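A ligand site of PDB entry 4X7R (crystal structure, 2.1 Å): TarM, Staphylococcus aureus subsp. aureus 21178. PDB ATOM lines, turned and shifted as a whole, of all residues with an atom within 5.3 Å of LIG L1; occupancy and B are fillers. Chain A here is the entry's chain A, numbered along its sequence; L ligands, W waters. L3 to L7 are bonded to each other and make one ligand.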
ATOM      1  N   LYS A  15       7.961  11.099  -6.074  1.00  0.00           N
ATOM      2  CA  LYS A  15       8.131   9.686  -6.448  1.00  0.00           C
ATOM      3  C   LYS A  15       8.025   8.678  -5.283  1.00  0.00           C
ATOM      4  O   LYS A  15       7.939   9.057  -4.116  1.00  0.00           O
ATOM      5  CB  LYS A  15       9.432   9.486  -7.268  1.00  0.00           C
ATOM      6  CG  LYS A  15       9.492  10.279  -8.586  1.00  0.00           C
ATOM      7  CD  LYS A  15       8.698   9.610  -9.700  1.00  0.00           C
ATOM      8  CE  LYS A  15       8.421  10.516 -10.865  1.00  0.00           C
ATOM      9  NZ  LYS A  15       7.410  11.563 -10.523  1.00  0.00           N
ATOM     10  N   GLY A  16       8.029   7.394  -5.652  1.00  0.00           N
ATOM     11  CA  GLY A  16       7.911   6.258  -4.749  1.00  0.00           C
ATOM     12  C   GLY A  16       9.214   5.587  -4.381  1.00  0.00           C
ATOM     13  O   GLY A  16      10.279   6.215  -4.327  1.00  0.00           O
ATOM     14  N   GLY A  17       9.115   4.286  -4.124  1.00  0.00           N
ATOM     15  CA  GLY A  17      10.189   3.471  -3.564  1.00  0.00           C
ATOM     16  C   GLY A  17      11.432   3.268  -4.379  1.00  0.00           C
ATOM     17  O   GLY A  17      12.507   3.149  -3.786  1.00  0.00           O
ATOM     18  N   MET A  18      11.329   3.176  -5.701  1.00  0.00           N
ATOM     19  CA  MET A  18      12.535   2.921  -6.502  1.00  0.00           C
ATOM     20  C   MET A  18      13.553   4.014  -6.381  1.00  0.00           C
ATOM     21  O   MET A  18      14.715   3.714  -6.139  1.00  0.00           O
ATOM     22  CB  MET A  18      12.210   2.604  -7.987  1.00  0.00           C
ATOM     23  CG  MET A  18      13.453   2.602  -8.919  1.00  0.00           C
ATOM     24  SD  MET A  18      13.155   2.006 -10.592  1.00  0.00           S
ATOM     25  CE  MET A  18      12.096   3.347 -11.232  1.00  0.00           C
ATOM     26  N   SER A  20      13.532   6.431  -4.053  1.00  0.00           N
ATOM     27  CA  SER A  20      13.767   6.490  -2.611  1.00  0.00           C
ATOM     28  C   SER A  20      14.920   5.496  -2.248  1.00  0.00           C
ATOM     29  O   SER A  20      15.872   5.881  -1.606  1.00  0.00           O
ATOM     30  CB  SER A  20      12.488   6.111  -1.862  1.00  0.00           C
ATOM     31  OG  SER A  20      12.605   6.177  -0.455  1.00  0.00           O
ATOM     32  N   LYS A  59      15.607  14.208   0.798  1.00  0.00           N
ATOM     33  CA  LYS A  59      15.361  12.938   0.095  1.00  0.00           C
ATOM     34  C   LYS A  59      16.657  12.491  -0.566  1.00  0.00           C
ATOM     35  O   LYS A  59      17.117  11.367  -0.374  1.00  0.00           O
ATOM     36  CB  LYS A  59      14.266  13.082  -0.983  1.00  0.00           C
ATOM     37  CG  LYS A  59      12.868  13.222  -0.425  1.00  0.00           C
ATOM     38  CD  LYS A  59      11.871  12.333  -1.153  1.00  0.00           C
ATOM     39  CE  LYS A  59      10.599  12.214  -0.340  1.00  0.00           C
ATOM     40  NZ  LYS A  59       9.613  11.326  -0.995  1.00  0.00           N
ATOM     41  N   ILE A 324       0.773   5.215   3.292  1.00  0.00           N
ATOM     42  CA  ILE A 324       1.645   6.115   2.540  1.00  0.00           C
ATOM     43  C   ILE A 324       2.199   5.375   1.328  1.00  0.00           C
ATOM     44  O   ILE A 324       3.031   4.485   1.500  1.00  0.00           O
ATOM     45  CB  ILE A 324       2.804   6.703   3.422  1.00  0.00           C
ATOM     46  CG1 ILE A 324       2.299   7.360   4.734  1.00  0.00           C
ATOM     47  CG2 ILE A 324       3.657   7.686   2.615  1.00  0.00           C
ATOM     48  CD1 ILE A 324       3.424   7.579   5.805  1.00  0.00           C
ATOM     49  N   SER A 325       1.743   5.725   0.112  1.00  0.00           N
ATOM     50  CA  SER A 325       2.206   5.087  -1.124  1.00  0.00           C
ATOM     51  C   SER A 325       1.944   5.933  -2.377  1.00  0.00           C
ATOM     52  O   SER A 325       1.269   6.972  -2.296  1.00  0.00           O
ATOM     53  CB  SER A 325       1.529   3.732  -1.311  1.00  0.00           C
ATOM     54  OG  SER A 325       0.191   3.862  -1.753  1.00  0.00           O
ATOM     55  N   ARG A 326       2.437   5.442  -3.535  1.00  0.00           N
ATOM     56  CA  ARG A 326       2.100   5.963  -4.862  1.00  0.00           C
ATOM     57  C   ARG A 326       0.656   5.453  -5.016  1.00  0.00           C
ATOM     58  O   ARG A 326       0.388   4.294  -4.651  1.00  0.00           O
ATOM     59  CB  ARG A 326       2.956   5.306  -5.950  1.00  0.00           C
ATOM     60  CG  ARG A 326       4.403   5.724  -6.006  1.00  0.00           C
ATOM     61  CD  ARG A 326       5.128   5.038  -7.157  1.00  0.00           C
ATOM     62  NE  ARG A 326       5.202   3.586  -6.979  1.00  0.00           N
ATOM     63  CZ  ARG A 326       4.792   2.694  -7.862  1.00  0.00           C
ATOM     64  NH1 ARG A 326       4.294   3.076  -9.023  1.00  0.00           N
ATOM     65  NH2 ARG A 326       4.888   1.391  -7.601  1.00  0.00           N
ATOM     66  N   LYS A 331      -1.451  -1.250  -5.570  1.00  0.00           N
ATOM     67  CA  LYS A 331      -1.591  -0.949  -4.146  1.00  0.00           C
ATOM     68  C   LYS A 331      -2.985  -1.293  -3.640  1.00  0.00           C
ATOM     69  O   LYS A 331      -3.191  -1.432  -2.427  1.00  0.00           O
ATOM     70  CB  LYS A 331      -1.225   0.518  -3.838  1.00  0.00           C
ATOM     71  CG  LYS A 331       0.187   0.916  -4.277  1.00  0.00           C
ATOM     72  CD  LYS A 331       1.306   0.265  -3.456  1.00  0.00           C
ATOM     73  CE  LYS A 331       2.633   0.534  -4.117  1.00  0.00           C
ATOM     74  NZ  LYS A 331       3.746  -0.129  -3.394  1.00  0.00           N
ATOM     75  N   TYR A 355      -1.955   8.947   2.228  1.00  0.00           N
ATOM     76  CA  TYR A 355      -1.014   9.880   1.610  1.00  0.00           C
ATOM     77  C   TYR A 355      -0.531   9.394   0.268  1.00  0.00           C
ATOM     78  O   TYR A 355      -0.387   8.181   0.054  1.00  0.00           O
ATOM     79  CB  TYR A 355       0.196  10.125   2.524  1.00  0.00           C
ATOM     80  CG  TYR A 355      -0.121  10.964   3.736  1.00  0.00           C
ATOM     81  CD1 TYR A 355      -0.592  10.380   4.917  1.00  0.00           C
ATOM     82  CD2 TYR A 355       0.059  12.349   3.726  1.00  0.00           C
ATOM     83  CE1 TYR A 355      -0.858  11.152   6.043  1.00  0.00           C
ATOM     84  CE2 TYR A 355      -0.206  13.122   4.853  1.00  0.00           C
ATOM     85  CZ  TYR A 355      -0.678  12.523   6.001  1.00  0.00           C
ATOM     86  OH  TYR A 355      -0.937  13.263   7.126  1.00  0.00           O
ATOM     87  N   GLY A 356      -0.232  10.336  -0.617  1.00  0.00           N
ATOM     88  CA  GLY A 356       0.292  10.079  -1.946  1.00  0.00           C
ATOM     89  C   GLY A 356      -0.556  10.660  -3.055  1.00  0.00           C
ATOM     90  O   GLY A 356      -1.583  11.293  -2.799  1.00  0.00           O
ATOM     91  N   GLY A 381      -3.003  13.821   0.318  1.00  0.00           N
ATOM     92  CA  GLY A 381      -2.007  14.215  -0.686  1.00  0.00           C
ATOM     93  C   GLY A 381      -0.608  13.674  -0.416  1.00  0.00           C
ATOM     94  O   GLY A 381      -0.392  12.963   0.558  1.00  0.00           O
ATOM     95  N   TYR A 382       0.354  14.023  -1.291  1.00  0.00           N
ATOM     96  CA  TYR A 382       1.743  13.575  -1.156  1.00  0.00           C
ATOM     97  C   TYR A 382       2.419  14.177   0.056  1.00  0.00           C
ATOM     98  O   TYR A 382       2.218  15.348   0.361  1.00  0.00           O
ATOM     99  CB  TYR A 382       2.556  13.874  -2.433  1.00  0.00           C
ATOM    100  CG  TYR A 382       3.903  13.169  -2.472  1.00  0.00           C
ATOM    101  CD1 TYR A 382       4.025  11.894  -3.017  1.00  0.00           C
ATOM    102  CD2 TYR A 382       5.032  13.765  -1.936  1.00  0.00           C
ATOM    103  CE1 TYR A 382       5.259  11.241  -3.039  1.00  0.00           C
ATOM    104  CE2 TYR A 382       6.272  13.125  -1.956  1.00  0.00           C
ATOM    105  CZ  TYR A 382       6.371  11.850  -2.497  1.00  0.00           C
ATOM    106  OH  TYR A 382       7.588  11.218  -2.517  1.00  0.00           O
ATOM    107  N   THR A 383       3.241  13.364   0.749  1.00  0.00           N
ATOM    108  CA  THR A 383       4.006  13.826   1.898  1.00  0.00           C
ATOM    109  C   THR A 383       5.511  13.740   1.637  1.00  0.00           C
ATOM    110  O   THR A 383       6.009  12.676   1.216  1.00  0.00           O
ATOM    111  CB  THR A 383       3.533  13.178   3.208  1.00  0.00           C
ATOM    112  OG1 THR A 383       4.242  13.787   4.282  1.00  0.00           O
ATOM    113  CG2 THR A 383       3.713  11.648   3.238  1.00  0.00           C
ATOM    114  N   THR A 384       6.230  14.856   1.849  1.00  0.00           N
ATOM    115  CA  THR A 384       7.684  14.947   1.698  1.00  0.00           C
ATOM    116  C   THR A 384       8.335  14.580   3.034  1.00  0.00           C
ATOM    117  O   THR A 384       9.548  14.401   3.095  1.00  0.00           O
ATOM    118  CB  THR A 384       8.141  16.317   1.151  1.00  0.00           C
ATOM    119  OG1 THR A 384       7.636  17.358   1.994  1.00  0.00           O
ATOM    120  CG2 THR A 384       7.708  16.546  -0.292  1.00  0.00           C
ATOM    121  N   PRO A 386       7.254  11.626   5.311  1.00  0.00           N
ATOM    122  CA  PRO A 386       6.464  10.452   5.751  1.00  0.00           C
ATOM    123  C   PRO A 386       6.739  10.031   7.194  1.00  0.00           C
ATOM    124  O   PRO A 386       5.798   9.632   7.875  1.00  0.00           O
ATOM    125  CB  PRO A 386       6.828   9.356   4.743  1.00  0.00           C
ATOM    126  CG  PRO A 386       8.142   9.762   4.170  1.00  0.00           C
ATOM    127  CD  PRO A 386       8.141  11.271   4.179  1.00  0.00           C
ATOM    128  N   GLU A 403       4.637  -6.657  -4.651  1.00  0.00           N
ATOM    129  CA  GLU A 403       5.765  -5.858  -4.178  1.00  0.00           C
ATOM    130  C   GLU A 403       7.065  -6.596  -4.503  1.00  0.00           C
ATOM    131  O   GLU A 403       7.082  -7.817  -4.685  1.00  0.00           O
ATOM    132  CB  GLU A 403       5.702  -5.607  -2.638  1.00  0.00           C
ATOM    133  CG  GLU A 403       4.550  -4.762  -2.100  1.00  0.00           C
ATOM    134  CD  GLU A 403       4.520  -3.322  -2.562  1.00  0.00           C
ATOM    135  OE1 GLU A 403       5.569  -2.797  -2.984  1.00  0.00           O
ATOM    136  OE2 GLU A 403       3.423  -2.715  -2.498  1.00  0.00           O
ATOM    137  N   GLY A 406       8.772  -3.541  -0.191  1.00  0.00           N
ATOM    138  CA  GLY A 406       7.815  -2.692   0.536  1.00  0.00           C
ATOM    139  C   GLY A 406       8.426  -1.807   1.583  1.00  0.00           C
ATOM    140  O   GLY A 406       8.299  -2.065   2.784  1.00  0.00           O
ATOM    141  N   LEU A 407       9.048  -0.722   1.152  1.00  0.00           N
ATOM    142  CA  LEU A 407       9.695   0.211   2.053  1.00  0.00           C
ATOM    143  C   LEU A 407       8.735   0.918   3.004  1.00  0.00           C
ATOM    144  O   LEU A 407       9.139   1.169   4.126  1.00  0.00           O
ATOM    145  CB  LEU A 407      10.578   1.223   1.302  1.00  0.00           C
ATOM    146  CG  LEU A 407      11.804   0.653   0.554  1.00  0.00           C
ATOM    147  CD1 LEU A 407      12.426   1.723  -0.355  1.00  0.00           C
ATOM    148  CD2 LEU A 407      12.869   0.139   1.547  1.00  0.00           C
ATOM    149  N   SER A 408       7.495   1.240   2.579  1.00  0.00           N
ATOM    150  CA  SER A 408       6.528   1.932   3.449  1.00  0.00           C
ATOM    151  C   SER A 408       6.167   1.084   4.656  1.00  0.00           C
ATOM    152  O   SER A 408       6.138   1.602   5.776  1.00  0.00           O
ATOM    153  CB  SER A 408       5.265   2.306   2.676  1.00  0.00           C
ATOM    154  OG  SER A 408       5.373   3.604   2.116  1.00  0.00           O
ATOM    155  N   MET A 409       5.956  -0.226   4.447  1.00  0.00           N
ATOM    156  CA  MET A 409       5.683  -1.188   5.526  1.00  0.00           C
ATOM    157  C   MET A 409       6.905  -1.236   6.472  1.00  0.00           C
ATOM    158  O   MET A 409       6.738  -1.118   7.686  1.00  0.00           O
ATOM    159  CB  MET A 409       5.402  -2.588   4.956  1.00  0.00           C
ATOM    160  CG  MET A 409       4.053  -2.688   4.249  1.00  0.00           C
ATOM    161  SD  MET A 409       3.721  -4.374   3.688  1.00  0.00           S
ATOM    162  CE  MET A 409       4.598  -4.382   2.102  1.00  0.00           C
ATOM    163  N   GLU A 411       9.284   1.096   6.772  1.00  0.00           N
ATOM    164  CA  GLU A 411       9.396   2.431   7.380  1.00  0.00           C
ATOM    165  C   GLU A 411       8.462   2.561   8.582  1.00  0.00           C
ATOM    166  O   GLU A 411       8.899   3.035   9.632  1.00  0.00           O
ATOM    167  CB  GLU A 411       9.104   3.540   6.353  1.00  0.00           C
ATOM    168  CG  GLU A 411      10.217   3.745   5.345  1.00  0.00           C
ATOM    169  CD  GLU A 411       9.841   4.581   4.142  1.00  0.00           C
ATOM    170  OE1 GLU A 411       8.843   5.335   4.220  1.00  0.00           O
ATOM    171  OE2 GLU A 411      10.532   4.468   3.101  1.00  0.00           O
HETATM  172  N1  LIG L   1       6.442   8.096  -0.308  1.00  0.00           N
HETATM  173  C1  LIG L   1       6.579   9.353   0.268  1.00  0.00           C
HETATM  174  N2  LIG L   1       5.427  10.102   0.315  1.00  0.00           N
HETATM  175  C2  LIG L   1       4.186   9.749  -0.168  1.00  0.00           C
HETATM  176  C3  LIG L   1       4.128   8.454  -0.797  1.00  0.00           C
HETATM  177  C4  LIG L   1       5.227   7.679  -0.844  1.00  0.00           C
HETATM  178  O1  LIG L   1       7.635   9.768   0.708  1.00  0.00           O
HETATM  179  O2  LIG L   1       3.230  10.530  -0.015  1.00  0.00           O
HETATM  180  C5  LIG L   1       7.610   7.191  -0.191  1.00  0.00           C
HETATM  181  C6  LIG L   1       7.580   6.286   1.041  1.00  0.00           C
HETATM  182  O3  LIG L   1       8.128   6.948   2.168  1.00  0.00           O
HETATM  183  C7  LIG L   1       8.454   5.119   0.580  1.00  0.00           C
HETATM  184  C8  LIG L   1       8.158   5.033  -0.911  1.00  0.00           C
HETATM  185  O4  LIG L   1       7.621   6.322  -1.307  1.00  0.00           O
HETATM  186  O5  LIG L   1       9.856   5.233   0.862  1.00  0.00           O
HETATM  187  C9  LIG L   1       7.220   3.931  -1.316  1.00  0.00           C
HETATM  188  O6  LIG L   1       7.964   2.695  -1.212  1.00  0.00           O
HETATM  189  P1  LIG L   1       7.367   1.226  -1.428  1.00  0.00           P
HETATM  190  O7  LIG L   1       8.479   0.268  -1.566  1.00  0.00           O
HETATM  191  O8  LIG L   1       6.486   0.878  -0.223  1.00  0.00           O
HETATM  192  O9  LIG L   1       6.491   1.238  -2.724  1.00  0.00           O
HETATM  193  P2  LIG L   1       6.775   1.713  -4.235  1.00  0.00           P
HETATM  194  O10 LIG L   1       8.201   1.406  -4.606  1.00  0.00           O
HETATM  195  O11 LIG L   1       6.526   3.224  -4.366  1.00  0.00           O
HETATM  196  O12 LIG L   1       5.861   0.948  -5.170  1.00  0.00           O
HETATM  197  O1  LG2 L   2       8.271   0.049 -11.328  1.00  0.00           O
HETATM  198  C1  LG2 L   2       9.520   0.749  -7.867  1.00  0.00           C
HETATM  199  C2  LG2 L   2       8.540   0.472  -8.976  1.00  0.00           C
HETATM  200  O2  LG2 L   2      10.904  -0.668  -5.513  1.00  0.00           O
HETATM  201  C3  LG2 L   2       9.228   0.223 -10.297  1.00  0.00           C
HETATM  202  C4  LG2 L   2      10.899  -0.531  -4.093  1.00  0.00           C
HETATM  203  C5  LG2 L   2      12.324  -0.227  -3.683  1.00  0.00           C
HETATM  204  C6  LG2 L   2      10.315  -1.804  -3.473  1.00  0.00           C
HETATM  205  O3  LG2 L   2      13.218  -1.255  -4.081  1.00  0.00           O
HETATM  206  C7  LG2 L   2       8.849  -1.901  -3.878  1.00  0.00           C
HETATM  207  O4  LG2 L   2      10.402  -1.747  -2.054  1.00  0.00           O
HETATM  208  O5  LG2 L   2       8.235  -3.076  -3.353  1.00  0.00           O
HETATM  209  O6  LG2 L   2       6.835  -3.520  -6.603  1.00  0.00           O
HETATM  210  C8  LG2 L   2       6.448  -2.410  -6.249  1.00  0.00           C
HETATM  211  C9  LG2 L   2       5.025  -1.992  -6.370  1.00  0.00           C
HETATM  212  N1  LG2 L   2       7.284  -1.513  -5.716  1.00  0.00           N
HETATM  213  C10 LG2 L   2       8.671  -1.800  -5.392  1.00  0.00           C
HETATM  214  C11 LG2 L   2       9.623  -0.835  -6.115  1.00  0.00           C
HETATM  215  O7  LG2 L   2       9.052   0.358  -6.571  1.00  0.00           O
HETATM  216  O8  LG2 L   2       7.651   1.586  -9.099  1.00  0.00           O
HETATM  217  C1  LG3 L   3       9.268   0.834 -30.717  1.00  0.00           C
HETATM  218  C2  LG3 L   3      10.066   1.264 -32.930  1.00  0.00           C
HETATM  219  C3  LG3 L   3       8.225   1.290 -29.669  1.00  0.00           C
HETATM  220  C4  LG3 L   3       8.782   2.424 -28.818  1.00  0.00           C
HETATM  221  C5  LG3 L   3      10.172   2.122 -28.206  1.00  0.00           C
HETATM  222  C6  LG3 L   3      11.137   1.569 -29.307  1.00  0.00           C
HETATM  223  C7  LG3 L   3      12.470   1.054 -28.718  1.00  0.00           C
HETATM  224  O1  LG3 L   3       9.426   1.817 -31.774  1.00  0.00           O
HETATM  225  N1  LG3 L   3       6.968   1.704 -30.278  1.00  0.00           N
HETATM  226  S1  LG3 L   3       5.788   0.401 -30.344  1.00  0.00           S
HETATM  227  O2  LG3 L   3       6.445  -0.825 -30.991  1.00  0.00           O
HETATM  228  O3  LG3 L   3       4.598   0.943 -31.149  1.00  0.00           O
HETATM  229  O4  LG3 L   3       5.333   0.044 -28.927  1.00  0.00           O
HETATM  230  O5  LG3 L   3       7.812   2.743 -27.822  1.00  0.00           O
HETATM  231  O6  LG3 L   3      10.666   3.374 -27.693  1.00  0.00           O
HETATM  232  O7  LG3 L   3      10.506   0.470 -30.040  1.00  0.00           O
HETATM  233  O8  LG3 L   3      13.250   0.408 -29.741  1.00  0.00           O
HETATM  234  S2  LG3 L   3      14.230   1.152 -30.670  1.00  0.00           S
HETATM  235  O9  LG3 L   3      14.506   0.270 -31.896  1.00  0.00           O
HETATM  236  O10 LG3 L   3      15.546   1.386 -29.925  1.00  0.00           O
HETATM  237  O11 LG3 L   3      13.653   2.501 -31.147  1.00  0.00           O
HETATM  238  C1  LG4 L   4      11.242   3.365 -26.376  1.00  0.00           C
HETATM  239  C2  LG4 L   4      11.948   4.721 -26.143  1.00  0.00           C
HETATM  240  C3  LG4 L   4      10.932   5.844 -25.702  1.00  0.00           C
HETATM  241  C4  LG4 L   4       9.933   5.366 -24.640  1.00  0.00           C
HETATM  242  C5  LG4 L   4       9.289   4.022 -25.059  1.00  0.00           C
HETATM  243  C6  LG4 L   4       8.320   3.485 -23.989  1.00  0.00           C
HETATM  244  O1  LG4 L   4      13.018   4.560 -25.173  1.00  0.00           O
HETATM  245  O2  LG4 L   4      10.188   6.365 -26.818  1.00  0.00           O
HETATM  246  O3  LG4 L   4      10.614   5.178 -23.404  1.00  0.00           O
HETATM  247  O4  LG4 L   4      10.355   3.052 -25.265  1.00  0.00           O
HETATM  248  O5  LG4 L   4       8.635   2.407 -23.440  1.00  0.00           O
HETATM  249  O6  LG4 L   4       7.300   4.171 -23.739  1.00  0.00           O
HETATM  250  S1  LG4 L   4      14.469   4.270 -25.586  1.00  0.00           S
HETATM  251  O7  LG4 L   4      14.588   3.179 -26.655  1.00  0.00           O
HETATM  252  O8  LG4 L   4      15.072   5.565 -26.109  1.00  0.00           O
HETATM  253  O9  LG4 L   4      15.250   3.786 -24.368  1.00  0.00           O
HETATM  254  N1  LG5 L   5      13.017   5.824 -22.132  1.00  0.00           N
HETATM  255  C1  LG5 L   5      10.677   6.404 -22.635  1.00  0.00           C
HETATM  256  S1  LG5 L   5      14.059   7.239 -22.182  1.00  0.00           S
HETATM  257  C2  LG5 L   5      11.716   6.193 -21.549  1.00  0.00           C
HETATM  258  S2  LG5 L   5       6.741   8.119 -19.091  1.00  0.00           S
HETATM  259  C3  LG5 L   5      11.217   5.122 -20.543  1.00  0.00           C
HETATM  260  O1  LG5 L   5      12.147   4.994 -19.444  1.00  0.00           O
HETATM  261  S3  LG5 L   5      12.916   3.688 -19.281  1.00  0.00           S
HETATM  262  C4  LG5 L   5       9.812   5.417 -20.005  1.00  0.00           C
HETATM  263  O2  LG5 L   5       9.426   4.248 -19.317  1.00  0.00           O
HETATM  264  C5  LG5 L   5       8.832   5.719 -21.196  1.00  0.00           C
HETATM  265  O3  LG5 L   5       9.404   6.768 -22.044  1.00  0.00           O
HETATM  266  C6  LG5 L   5       7.484   6.291 -20.763  1.00  0.00           C
HETATM  267  O4  LG5 L   5       7.746   7.486 -20.033  1.00  0.00           O
HETATM  268  O5  LG5 L   5      14.406   7.655 -20.750  1.00  0.00           O
HETATM  269  O6  LG5 L   5      15.294   6.839 -22.970  1.00  0.00           O
HETATM  270  O7  LG5 L   5      13.346   8.405 -22.869  1.00  0.00           O
HETATM  271  O8  LG5 L   5       7.457   9.218 -18.301  1.00  0.00           O
HETATM  272  O9  LG5 L   5       5.594   8.692 -19.932  1.00  0.00           O
HETATM  273  O10 LG5 L   5       6.201   7.063 -18.116  1.00  0.00           O
HETATM  274  O11 LG5 L   5      11.884   2.573 -19.177  1.00  0.00           O
HETATM  275  O12 LG5 L   5      13.764   3.694 -18.014  1.00  0.00           O
HETATM  276  O13 LG5 L   5      13.806   3.439 -20.497  1.00  0.00           O
HETATM  277  C1  LG6 L   6       8.731   4.599 -18.111  1.00  0.00           C
HETATM  278  C2  LG6 L   6       7.597   3.560 -17.888  1.00  0.00           C
HETATM  279  C3  LG6 L   6       6.898   3.816 -16.549  1.00  0.00           C
HETATM  280  C4  LG6 L   6       7.939   4.016 -15.378  1.00  0.00           C
HETATM  281  C5  LG6 L   6       9.015   5.059 -15.803  1.00  0.00           C
HETATM  282  C6  LG6 L   6      10.093   5.291 -14.716  1.00  0.00           C
HETATM  283  O1  LG6 L   6       6.651   3.660 -18.947  1.00  0.00           O
HETATM  284  O2  LG6 L   6       6.010   2.718 -16.264  1.00  0.00           O
HETATM  285  O3  LG6 L   6       7.227   4.549 -14.253  1.00  0.00           O
HETATM  286  O4  LG6 L   6       9.669   4.619 -17.027  1.00  0.00           O
HETATM  287  O5  LG6 L   6      10.919   4.366 -14.523  1.00  0.00           O
HETATM  288  O6  LG6 L   6      10.116   6.417 -14.164  1.00  0.00           O
HETATM  289  C1  LG7 L   7       7.175   3.621 -13.142  1.00  0.00           C
HETATM  290  C2  LG7 L   7       5.782   3.751 -12.461  1.00  0.00           C
HETATM  291  C3  LG7 L   7       5.592   5.146 -11.779  1.00  0.00           C
HETATM  292  C4  LG7 L   7       6.807   5.542 -10.920  1.00  0.00           C
HETATM  293  C5  LG7 L   7       8.141   5.316 -11.683  1.00  0.00           C
HETATM  294  C6  LG7 L   7       9.350   5.640 -10.811  1.00  0.00           C
HETATM  295  N1  LG7 L   7       4.714   3.484 -13.429  1.00  0.00           N
HETATM  296  O1  LG7 L   7       4.421   5.137 -10.936  1.00  0.00           O
HETATM  297  O2  LG7 L   7       6.711   6.920 -10.516  1.00  0.00           O
HETATM  298  O3  LG7 L   7       8.238   3.942 -12.198  1.00  0.00           O
HETATM  299  O4  LG7 L   7       9.294   4.797  -9.658  1.00  0.00           O
HETATM  300  S1  LG7 L   7       4.019   1.914 -13.208  1.00  0.00           S
HETATM  301  O5  LG7 L   7       3.316   1.858 -11.854  1.00  0.00           O
HETATM  302  O6  LG7 L   7       5.111   0.826 -13.264  1.00  0.00           O
HETATM  303  O7  LG7 L   7       3.019   1.699 -14.348  1.00  0.00           O
HETATM  304  S2  LG7 L   7       9.254   5.402  -8.264  1.00  0.00           S
HETATM  305  O8  LG7 L   7       8.947   4.256  -7.294  1.00  0.00           O
HETATM  306  O9  LG7 L   7       8.199   6.491  -8.114  1.00  0.00           O
HETATM  307  O10 LG7 L   7      10.644   5.984  -8.011  1.00  0.00           O
HETATM  308  O   HOH W   1       3.930   1.479  -0.953  1.00  0.00           O
HETATM  309  O   HOH W   2       4.429   3.210  -2.921  1.00  0.00           O
HETATM  310  O   HOH W   3       5.296  -1.014   1.157  1.00  0.00           O
HETATM  311  O   HOH W   4       6.187   5.385   4.320  1.00  0.00           O
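An oxygen (O5) of LIG L1 sits at hydrogen-bond distance from the side-chain carboxylate (OE2) of Glu 411, at 2.5 Å.
NH2 of Arg 326 is in salt-bridge range of O12 of LIG L1, 2.7 Å away.
O2 of LIG L1 lies within hydrogen-bond range of N of Thr 383 (2.9 Å).
The backbone carbonyl oxygen of Thr 383 sits at hydrogen-bond distance from a nitrogen (N2) of LIG L1.
N of Gly 17 sits at hydrogen-bond distance from O11 of LIG L1, at 2.8 Å.
The backbone NH (N) of Leu 407 is in hydrogen-bond range of an oxygen (O7) of LIG L1, at 2.9 Å.
NZ of Lys 331 is in salt-bridge range of O12 of LIG L1, at 3.0 Å.
An oxygen (O8) of LIG L1 is in hydrogen-bond range of the backbone NH (N) of Ser 408 (3.0 Å).
The side-chain amino group of Lys 59 lies within hydrogen-bond range of an oxygen (O1) of LIG L1 (3.0 Å).
The side-chain hydroxyl (OG) of Ser 20 is in hydrogen-bond range of an oxygen (O5) of LIG L1.
O8 of LG2 L2 is in hydrogen-bond range of NH2 of Arg 326 (3.1 Å).
The backbone NH (N) of Gly 406 sits at hydrogen-bond distance from an oxygen (O4) of LG2 L2, 3.1 Å away.
The side-chain carboxylate of Glu 403 is in hydrogen-bond range of an oxygen (O5) of LG2 L2 (2.7 Å).
O5 of LG7 L7 lies within salt-bridge range of NH1 of Arg 326, 3.2 Å away.
An oxygen (O8) of LG7 L7 is in hydrogen-bond range of the backbone NH (N) of Gly 17 (3.2 Å).
An oxygen (O9) of LG7 L7 is in hydrogen-bond range of the backbone NH (N) of Gly 16 (2.6 Å).
An oxygen (O8) of LG7 L7 lies within hydrogen-bond range of the backbone NH (N) of Met 18.
An oxygen (O7) of LIG L1 lies within hydrogen-bond range of an oxygen (O4) of LG2 L2 (2.8 Å).
An oxygen (O8) of LG7 L7 is in hydrogen-bond range of an oxygen (O8) of LG2 L2.
Lys 15 touches LIG L1.
CA of Gly 16 touches O11 of LIG L1, at 3.4 Å.
Met 18 touches LIG L1 (N to O10, 3.8 Å).
CG2 of Ile 324 touches C2 of LIG L1, at 3.5 Å.
O of Ser 325 touches C3 of LIG L1, 3.6 Å away.
Tyr 355 touches LIG L1 (C to O2, 3.9 Å).
Gly 356 touches LIG L1.
Tyr 382 touches LIG L1 (CD1 to O2, 3.4 Å).
Pro 386 touches LIG L1 (CG to O3, 3.5 Å).
Gly 406 touches LIG L1 (CA to O7, 3.7 Å).
Hydrophobic or aromatic side chains within 4 Å of LIG L1: Ile 324, Tyr 355, Tyr 382, Pro 386 and Leu 407.
The side-chain amino group (NZ) of Lys 331 is in salt-bridge range of the side-chain carboxylate (OE2) of Glu 403.
The backbone carbonyl oxygen (O) of Ile 324 is in hydrogen-bond range of the side-chain hydroxyl (OG) of Ser 408 (2.6 Å).
The side-chain hydroxyl (OH) of Tyr 382 lies within hydrogen-bond range of the side-chain amino group (NZ) of Lys 59, 2.5 Å away.
O of Lys 15 lies within hydrogen-bond range of OH of Tyr 382.
The backbone carbonyl oxygen (O) of Gly 381 sits at hydrogen-bond distance from the backbone NH (N) of Gly 356 (2.9 Å).
O of Tyr 355 lies within hydrogen-bond range of N of Ser 325, 3.3 Å away.
Water W2 lies within hydrogen-bond range of O11 of LIG L1, N of Arg 326 and NZ of Lys 331.
Water W3 lies within hydrogen-bond range of O8 of LIG L1, N of Met 409 and N of Ser 408.
Water W1 lies within hydrogen-bond range of O8 of LIG L1 (2.7 Å) and NZ of Lys 331 (2.9 Å).
Water W4 lies within hydrogen-bond range of the side-chain carboxylate of Glu 411, the side-chain hydroxyl of Ser 408 and an oxygen (O3) of LIG L1.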
